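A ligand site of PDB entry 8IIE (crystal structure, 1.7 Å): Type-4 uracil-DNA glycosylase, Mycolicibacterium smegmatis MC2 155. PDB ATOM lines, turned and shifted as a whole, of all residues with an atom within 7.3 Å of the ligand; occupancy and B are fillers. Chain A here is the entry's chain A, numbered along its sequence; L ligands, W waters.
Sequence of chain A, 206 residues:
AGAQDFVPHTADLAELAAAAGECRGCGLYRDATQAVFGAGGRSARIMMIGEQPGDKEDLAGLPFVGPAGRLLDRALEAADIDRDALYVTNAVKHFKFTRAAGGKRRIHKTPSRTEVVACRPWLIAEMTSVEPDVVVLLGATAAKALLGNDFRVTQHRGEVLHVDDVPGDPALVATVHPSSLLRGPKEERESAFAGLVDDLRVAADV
O of Gln 52 sits at hydrogen-bond distance from N2 of the ligand (2.9 Å).
A ring nitrogen (NE2) of His 177 sits at hydrogen-bond distance from an oxygen (O1) of the ligand (2.8 Å).
The backbone NH of Glu 51 is in hydrogen-bond range of an oxygen (O1) of the ligand (2.9 Å).
A nitrogen (N2) of the ligand lies within hydrogen-bond range of the side-chain amide oxygen of Asn 90, at 2.8 Å.
An oxygen (O2) of the ligand lies within hydrogen-bond range of the backbone NH (N) of Phe 64, at 2.9 Å.
N of Gln 52 sits at hydrogen-bond distance from O1 of the ligand (3.5 Å).
The backbone carbonyl oxygen (O) of Pro 63 is in hydrogen-bond range of the guanidinium group (NH2) of Arg 83, 2.9 Å away.
The side-chain carboxylate (OE1) of Glu 57 is in hydrogen-bond range of the backbone NH (N) of Gly 54 (2.9 Å).
N of Gly 50 lies within hydrogen-bond range of O of Thr 89.
The backbone NH (N) of Val 92 sits at hydrogen-bond distance from the backbone carbonyl oxygen (O) of Glu 51.
The backbone NH (N) of Ser 179 sits at hydrogen-bond distance from a ring nitrogen (ND1) of His 177 (3.0 Å).
NH2 of Arg 83 is in hydrogen-bond range of O of Phe 64, at 3.0 Å.
The side-chain amide oxygen (OD1) of Asn 90 is in hydrogen-bond range of the backbone NH (N) of Gln 52, at 3.4 Å.
OE2 of Glu 51 sits at hydrogen-bond distance from NE2 of Gln 52 (3.1 Å).
Residues that only touch the ligand: Gly 50, Glu 57 and Pro 63.
Hydrophobic or aromatic side chains that line the ligand: Pro 63, Phe 64 and His 177.
Of the 28 residues printed, 8 come within 4 Å of the ligand.
Along chain A the residues within 4 Å of the ligand span positions 50 to 177.
The nearest printed residue that does not touch the ligand is Pro 53 (4.1 Å).
Water W1 lies within hydrogen-bond range of a nitrogen (N1) of the ligand (2.8 Å) and the side-chain hydroxyl (OG) of Ser 179 (3.0 Å).
Water W2 lies within hydrogen-bond range of the backbone carbonyl oxygen (O) of Gln 52 (3.1 Å), a nitrogen (N1) of the ligand (3.3 Å) and the backbone NH (N) of Gly 54 (3.5 Å).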
ATOM      1  N   VAL A  36      27.452  12.820  10.297  1.00  0.00           N
ATOM      2  CA  VAL A  36      26.739  12.080  11.368  1.00  0.00           C
ATOM      3  C   VAL A  36      25.319  11.856  10.872  1.00  0.00           C
ATOM      4  O   VAL A  36      24.542  12.784  10.834  1.00  0.00           O
ATOM      5  CB  VAL A  36      26.775  12.844  12.706  1.00  0.00           C
ATOM      6  CG1 VAL A  36      25.999  12.118  13.793  1.00  0.00           C
ATOM      7  CG2 VAL A  36      28.213  13.089  13.144  1.00  0.00           C
ATOM      8  N   ILE A  49      14.366  15.111  15.175  1.00  0.00           N
ATOM      9  CA  ILE A  49      15.392  15.831  14.369  1.00  0.00           C
ATOM     10  C   ILE A  49      15.954  17.024  15.169  1.00  0.00           C
ATOM     11  O   ILE A  49      15.188  17.852  15.570  1.00  0.00           O
ATOM     12  CB  ILE A  49      14.768  16.344  13.051  1.00  0.00           C
ATOM     13  CG1 ILE A  49      14.056  15.228  12.281  1.00  0.00           C
ATOM     14  CG2 ILE A  49      15.806  17.031  12.172  1.00  0.00           C
ATOM     15  CD1 ILE A  49      13.387  15.706  11.017  1.00  0.00           C
ATOM     16  N   GLY A  50      17.259  17.014  15.385  1.00  0.00           N
ATOM     17  CA  GLY A  50      17.927  18.166  16.001  1.00  0.00           C
ATOM     18  C   GLY A  50      18.543  19.078  14.931  1.00  0.00           C
ATOM     19  O   GLY A  50      18.186  18.989  13.794  1.00  0.00           O
ATOM     20  N   GLU A  51      19.488  19.916  15.334  1.00  0.00           N
ATOM     21  CA  GLU A  51      20.051  20.921  14.386  1.00  0.00           C
ATOM     22  C   GLU A  51      21.243  20.345  13.625  1.00  0.00           C
ATOM     23  O   GLU A  51      21.229  20.354  12.428  1.00  0.00           O
ATOM     24  CB  GLU A  51      20.556  22.112  15.200  1.00  0.00           C
ATOM     25  CG  GLU A  51      21.300  23.147  14.402  1.00  0.00           C
ATOM     26  CD  GLU A  51      21.613  24.393  15.191  1.00  0.00           C
ATOM     27  OE1 GLU A  51      20.768  25.290  15.216  1.00  0.00           O
ATOM     28  OE2 GLU A  51      22.690  24.452  15.782  1.00  0.00           O
ATOM     29  N   GLN A  52      22.216  19.878  14.387  1.00  0.00           N
ATOM     30  CA  GLN A  52      23.474  19.383  13.786  1.00  0.00           C
ATOM     31  C   GLN A  52      24.254  18.617  14.850  1.00  0.00           C
ATOM     32  O   GLN A  52      24.031  18.800  16.028  1.00  0.00           O
ATOM     33  CB  GLN A  52      24.345  20.561  13.362  1.00  0.00           C
ATOM     34  CG  GLN A  52      24.810  21.399  14.537  1.00  0.00           C
ATOM     35  CD  GLN A  52      25.746  22.485  14.093  1.00  0.00           C
ATOM     36  OE1 GLN A  52      26.706  22.233  13.379  1.00  0.00           O
ATOM     37  NE2 GLN A  52      25.447  23.703  14.490  1.00  0.00           N
ATOM     38  N   PRO A  53      25.192  17.751  14.443  1.00  0.00           N
ATOM     39  CA  PRO A  53      26.018  17.093  15.425  1.00  0.00           C
ATOM     40  C   PRO A  53      26.878  18.137  16.129  1.00  0.00           C
ATOM     41  O   PRO A  53      27.257  19.069  15.496  1.00  0.00           O
ATOM     42  CB  PRO A  53      27.004  16.242  14.612  1.00  0.00           C
ATOM     43  CG  PRO A  53      26.860  16.737  13.191  1.00  0.00           C
ATOM     44  CD  PRO A  53      25.473  17.316  13.081  1.00  0.00           C
ATOM     45  N   GLY A  54      27.150  17.937  17.411  1.00  0.00           N
ATOM     46  CA  GLY A  54      28.080  18.825  18.117  1.00  0.00           C
ATOM     47  C   GLY A  54      29.463  18.214  18.188  1.00  0.00           C
ATOM     48  O   GLY A  54      29.738  17.302  17.446  1.00  0.00           O
ATOM     49  N   ASP A  55      30.262  18.726  19.111  1.00  0.00           N
ATOM     50  CA  ASP A  55      31.671  18.292  19.233  1.00  0.00           C
ATOM     51  C   ASP A  55      31.761  16.777  19.466  1.00  0.00           C
ATOM     52  O   ASP A  55      32.524  16.107  18.764  1.00  0.00           O
ATOM     53  CB  ASP A  55      32.327  19.157  20.310  1.00  0.00           C
ATOM     54  CG  ASP A  55      33.825  18.943  20.529  1.00  0.00           C
ATOM     55  OD1 ASP A  55      34.424  18.131  19.828  1.00  0.00           O
ATOM     56  OD2 ASP A  55      34.364  19.608  21.409  1.00  0.00           O
ATOM     57  N   GLU A  57      29.447  14.410  19.038  1.00  0.00           N
ATOM     58  CA  GLU A  57      28.834  13.639  17.921  1.00  0.00           C
ATOM     59  C   GLU A  57      29.774  13.553  16.721  1.00  0.00           C
ATOM     60  O   GLU A  57      29.798  12.537  16.062  1.00  0.00           O
ATOM     61  CB  GLU A  57      27.526  14.335  17.507  1.00  0.00           C
ATOM     62  CG  GLU A  57      26.434  14.264  18.557  1.00  0.00           C
ATOM     63  CD  GLU A  57      26.562  15.150  19.770  1.00  0.00           C
ATOM     64  OE1 GLU A  57      27.310  16.123  19.697  1.00  0.00           O
ATOM     65  OE2 GLU A  57      25.916  14.864  20.777  1.00  0.00           O
ATOM     66  N   LEU A  62      27.623   9.488  15.986  1.00  0.00           N
ATOM     67  CA  LEU A  62      26.235   9.205  16.429  1.00  0.00           C
ATOM     68  C   LEU A  62      25.619  10.503  16.938  1.00  0.00           C
ATOM     69  O   LEU A  62      26.311  11.310  17.466  1.00  0.00           O
ATOM     70  CB  LEU A  62      26.295   8.234  17.607  1.00  0.00           C
ATOM     71  CG  LEU A  62      26.701   6.801  17.300  1.00  0.00           C
ATOM     72  CD1 LEU A  62      27.047   6.055  18.578  1.00  0.00           C
ATOM     73  CD2 LEU A  62      25.600   6.090  16.536  1.00  0.00           C
ATOM     74  N   PRO A  63      24.308  10.688  16.765  1.00  0.00           N
ATOM     75  CA  PRO A  63      23.685  11.868  17.302  1.00  0.00           C
ATOM     76  C   PRO A  63      23.363  11.869  18.807  1.00  0.00           C
ATOM     77  O   PRO A  63      23.222  10.840  19.362  1.00  0.00           O
ATOM     78  CB  PRO A  63      22.369  11.935  16.501  1.00  0.00           C
ATOM     79  CG  PRO A  63      22.062  10.495  16.156  1.00  0.00           C
ATOM     80  CD  PRO A  63      23.418   9.837  15.980  1.00  0.00           C
ATOM     81  N   PHE A  64      23.274  13.069  19.380  1.00  0.00           N
ATOM     82  CA  PHE A  64      22.789  13.219  20.785  1.00  0.00           C
ATOM     83  C   PHE A  64      23.535  12.294  21.754  1.00  0.00           C
ATOM     84  O   PHE A  64      22.887  11.538  22.446  1.00  0.00           O
ATOM     85  CB  PHE A  64      21.265  13.146  20.812  1.00  0.00           C
ATOM     86  CG  PHE A  64      20.572  14.401  20.358  1.00  0.00           C
ATOM     87  CD1 PHE A  64      20.646  15.552  21.124  1.00  0.00           C
ATOM     88  CD2 PHE A  64      19.859  14.440  19.183  1.00  0.00           C
ATOM     89  CE1 PHE A  64      19.995  16.714  20.719  1.00  0.00           C
ATOM     90  CE2 PHE A  64      19.216  15.594  18.771  1.00  0.00           C
ATOM     91  CZ  PHE A  64      19.282  16.729  19.546  1.00  0.00           C
ATOM     92  N   VAL A  65      24.853  12.466  21.815  1.00  0.00           N
ATOM     93  CA  VAL A  65      25.679  11.649  22.757  1.00  0.00           C
ATOM     94  C   VAL A  65      26.366  12.568  23.781  1.00  0.00           C
ATOM     95  O   VAL A  65      27.072  12.042  24.627  1.00  0.00           O
ATOM     96  CB  VAL A  65      26.700  10.779  22.010  1.00  0.00           C
ATOM     97  CG1 VAL A  65      26.027   9.668  21.213  1.00  0.00           C
ATOM     98  CG2 VAL A  65      27.600  11.610  21.113  1.00  0.00           C
ATOM     99  N   GLY A  66      26.157  13.871  23.688  1.00  0.00           N
ATOM    100  CA  GLY A  66      26.745  14.772  24.679  1.00  0.00           C
ATOM    101  C   GLY A  66      25.709  15.230  25.704  1.00  0.00           C
ATOM    102  O   GLY A  66      24.721  14.557  25.882  1.00  0.00           O
ATOM    103  N   PRO A  67      25.968  16.363  26.374  1.00  0.00           N
ATOM    104  CA  PRO A  67      25.080  16.850  27.425  1.00  0.00           C
ATOM    105  C   PRO A  67      23.610  17.039  27.004  1.00  0.00           C
ATOM    106  O   PRO A  67      22.754  16.704  27.759  1.00  0.00           O
ATOM    107  CB  PRO A  67      25.731  18.171  27.837  1.00  0.00           C
ATOM    108  CG  PRO A  67      27.193  17.985  27.486  1.00  0.00           C
ATOM    109  CD  PRO A  67      27.166  17.185  26.202  1.00  0.00           C
ATOM    110  N   ALA A  68      23.407  17.610  25.828  1.00  0.00           N
ATOM    111  CA  ALA A  68      22.020  17.781  25.335  1.00  0.00           C
ATOM    112  C   ALA A  68      21.377  16.399  25.160  1.00  0.00           C
ATOM    113  O   ALA A  68      20.204  16.258  25.442  1.00  0.00           O
ATOM    114  CB  ALA A  68      22.041  18.539  24.043  1.00  0.00           C
ATOM    115  N   GLY A  69      22.152  15.419  24.693  1.00  0.00           N
ATOM    116  CA  GLY A  69      21.625  14.059  24.525  1.00  0.00           C
ATOM    117  C   GLY A  69      21.251  13.418  25.853  1.00  0.00           C
ATOM    118  O   GLY A  69      20.291  12.672  25.900  1.00  0.00           O
ATOM    119  N   ARG A  83      14.423   5.238  23.648  1.00  0.00           N
ATOM    120  CA  ARG A  83      15.266   5.866  22.578  1.00  0.00           C
ATOM    121  C   ARG A  83      15.623   4.817  21.521  1.00  0.00           C
ATOM    122  O   ARG A  83      15.837   5.184  20.366  1.00  0.00           O
ATOM    123  CB  ARG A  83      16.534   6.474  23.166  1.00  0.00           C
ATOM    124  CG  ARG A  83      17.266   7.395  22.191  1.00  0.00           C
ATOM    125  CD  ARG A  83      18.568   7.875  22.802  1.00  0.00           C
ATOM    126  NE  ARG A  83      19.450   8.373  21.778  1.00  0.00           N
ATOM    127  CZ  ARG A  83      20.320   9.355  21.947  1.00  0.00           C
ATOM    128  NH1 ARG A  83      20.417   9.966  23.104  1.00  0.00           N
ATOM    129  NH2 ARG A  83      21.093   9.718  20.941  1.00  0.00           N
ATOM    130  N   VAL A  88      16.678   8.916  15.270  1.00  0.00           N
ATOM    131  CA  VAL A  88      17.143  10.252  15.724  1.00  0.00           C
ATOM    132  C   VAL A  88      18.159  10.769  14.720  1.00  0.00           C
ATOM    133  O   VAL A  88      19.118  10.082  14.455  1.00  0.00           O
ATOM    134  CB  VAL A  88      17.743  10.174  17.137  1.00  0.00           C
ATOM    135  CG1 VAL A  88      18.252  11.522  17.606  1.00  0.00           C
ATOM    136  CG2 VAL A  88      16.765   9.584  18.133  1.00  0.00           C
ATOM    137  N   THR A  89      17.928  11.994  14.238  1.00  0.00           N
ATOM    138  CA  THR A  89      18.862  12.597  13.271  1.00  0.00           C
ATOM    139  C   THR A  89      18.912  14.121  13.473  1.00  0.00           C
ATOM    140  O   THR A  89      18.468  14.600  14.520  1.00  0.00           O
ATOM    141  CB  THR A  89      18.469  12.215  11.838  1.00  0.00           C
ATOM    142  OG1 THR A  89      19.507  12.509  10.897  1.00  0.00           O
ATOM    143  CG2 THR A  89      17.139  12.791  11.410  1.00  0.00           C
ATOM    144  N   ASN A  90      19.479  14.803  12.482  1.00  0.00           N
ATOM    145  CA  ASN A  90      19.688  16.265  12.578  1.00  0.00           C
ATOM    146  C   ASN A  90      19.398  16.885  11.208  1.00  0.00           C
ATOM    147  O   ASN A  90      19.563  16.192  10.225  1.00  0.00           O
ATOM    148  CB  ASN A  90      21.143  16.572  12.939  1.00  0.00           C
ATOM    149  CG  ASN A  90      21.432  16.269  14.388  1.00  0.00           C
ATOM    150  OD1 ASN A  90      20.814  16.864  15.264  1.00  0.00           O
ATOM    151  ND2 ASN A  90      22.331  15.342  14.651  1.00  0.00           N
ATOM    152  N   ALA A  91      19.100  18.169  11.206  1.00  0.00           N
ATOM    153  CA  ALA A  91      18.824  18.903   9.944  1.00  0.00           C
ATOM    154  C   ALA A  91      20.085  18.986   9.067  1.00  0.00           C
ATOM    155  O   ALA A  91      19.941  18.878   7.857  1.00  0.00           O
ATOM    156  CB  ALA A  91      18.268  20.264  10.259  1.00  0.00           C
ATOM    157  N   VAL A  92      21.236  19.228   9.696  1.00  0.00           N
ATOM    158  CA  VAL A  92      22.534  19.220   8.957  1.00  0.00           C
ATOM    159  C   VAL A  92      23.410  18.086   9.500  1.00  0.00           C
ATOM    160  O   VAL A  92      23.348  17.852  10.694  1.00  0.00           O
ATOM    161  CB  VAL A  92      23.250  20.582   8.868  1.00  0.00           C
ATOM    162  CG1 VAL A  92      22.287  21.726   8.582  1.00  0.00           C
ATOM    163  CG2 VAL A  92      24.197  20.903  10.004  1.00  0.00           C
ATOM    164  N   HIS A 108      29.565  24.978  18.518  1.00  0.00           N
ATOM    165  CA  HIS A 108      28.668  24.906  17.339  1.00  0.00           C
ATOM    166  C   HIS A 108      28.295  26.301  16.860  1.00  0.00           C
ATOM    167  O   HIS A 108      28.087  27.197  17.677  1.00  0.00           O
ATOM    168  CB  HIS A 108      27.416  24.062  17.581  1.00  0.00           C
ATOM    169  CG  HIS A 108      26.676  24.358  18.845  1.00  0.00           C
ATOM    170  ND1 HIS A 108      25.631  25.251  18.888  1.00  0.00           N
ATOM    171  CD2 HIS A 108      26.812  23.870  20.091  1.00  0.00           C
ATOM    172  CE1 HIS A 108      25.159  25.314  20.102  1.00  0.00           C
ATOM    173  NE2 HIS A 108      25.857  24.475  20.866  1.00  0.00           N
ATOM    174  N   LEU A 138      13.310  19.240  17.204  1.00  0.00           N
ATOM    175  CA  LEU A 138      13.957  19.753  18.424  1.00  0.00           C
ATOM    176  C   LEU A 138      14.655  21.061  18.082  1.00  0.00           C
ATOM    177  O   LEU A 138      15.747  21.032  17.530  1.00  0.00           O
ATOM    178  CB  LEU A 138      14.945  18.711  18.962  1.00  0.00           C
ATOM    179  CG  LEU A 138      14.361  17.330  19.296  1.00  0.00           C
ATOM    180  CD1 LEU A 138      15.469  16.289  19.308  1.00  0.00           C
ATOM    181  CD2 LEU A 138      13.677  17.361  20.645  1.00  0.00           C
ATOM    182  N   HIS A 177      14.800  22.921  21.996  1.00  0.00           N
ATOM    183  CA  HIS A 177      16.019  22.109  21.826  1.00  0.00           C
ATOM    184  C   HIS A 177      16.563  21.761  23.216  1.00  0.00           C
ATOM    185  O   HIS A 177      16.638  22.639  24.049  1.00  0.00           O
ATOM    186  CB  HIS A 177      17.081  22.940  21.119  1.00  0.00           C
ATOM    187  CG  HIS A 177      18.169  22.088  20.576  1.00  0.00           C
ATOM    188  ND1 HIS A 177      19.093  21.464  21.391  1.00  0.00           N
ATOM    189  CD2 HIS A 177      18.460  21.706  19.322  1.00  0.00           C
ATOM    190  CE1 HIS A 177      19.915  20.757  20.651  1.00  0.00           C
ATOM    191  NE2 HIS A 177      19.560  20.893  19.383  1.00  0.00           N
ATOM    192  N   PRO A 178      16.890  20.484  23.485  1.00  0.00           N
ATOM    193  CA  PRO A 178      17.427  20.096  24.771  1.00  0.00           C
ATOM    194  C   PRO A 178      18.599  20.952  25.274  1.00  0.00           C
ATOM    195  O   PRO A 178      18.724  21.125  26.427  1.00  0.00           O
ATOM    196  CB  PRO A 178      17.859  18.620  24.589  1.00  0.00           C
ATOM    197  CG  PRO A 178      17.550  18.259  23.155  1.00  0.00           C
ATOM    198  CD  PRO A 178      16.658  19.346  22.602  1.00  0.00           C
ATOM    199  N   SER A 179      19.400  21.486  24.357  1.00  0.00           N
ATOM    200  CA  SER A 179      20.559  22.333  24.740  1.00  0.00           C
ATOM    201  C   SER A 179      20.078  23.565  25.498  1.00  0.00           C
ATOM    202  O   SER A 179      20.794  24.051  26.345  1.00  0.00           O
ATOM    203  CB  SER A 179      21.337  22.751  23.523  1.00  0.00           C
ATOM    204  OG  SER A 179      22.077  21.679  22.993  1.00  0.00           O
HETATM  205  N1  LIG L   1      22.734  18.953  19.231  1.00  0.00           N
HETATM  206  C1  LIG L   1      21.973  18.633  18.148  1.00  0.00           C
HETATM  207  O1  LIG L   1      21.160  19.412  17.646  1.00  0.00           O
HETATM  208  N2  LIG L   1      22.115  17.365  17.679  1.00  0.00           N
HETATM  209  C2  LIG L   1      22.985  16.416  18.170  1.00  0.00           C
HETATM  210  O2  LIG L   1      23.057  15.318  17.610  1.00  0.00           O
HETATM  211  C3  LIG L   1      23.724  16.802  19.331  1.00  0.00           C
HETATM  212  C4  LIG L   1      23.584  18.055  19.819  1.00  0.00           C
HETATM  213  O   HOH W   1      23.067  21.577  20.200  1.00  0.00           O
HETATM  214  O   HOH W   2      25.283  20.792  18.110  1.00  0.00           O
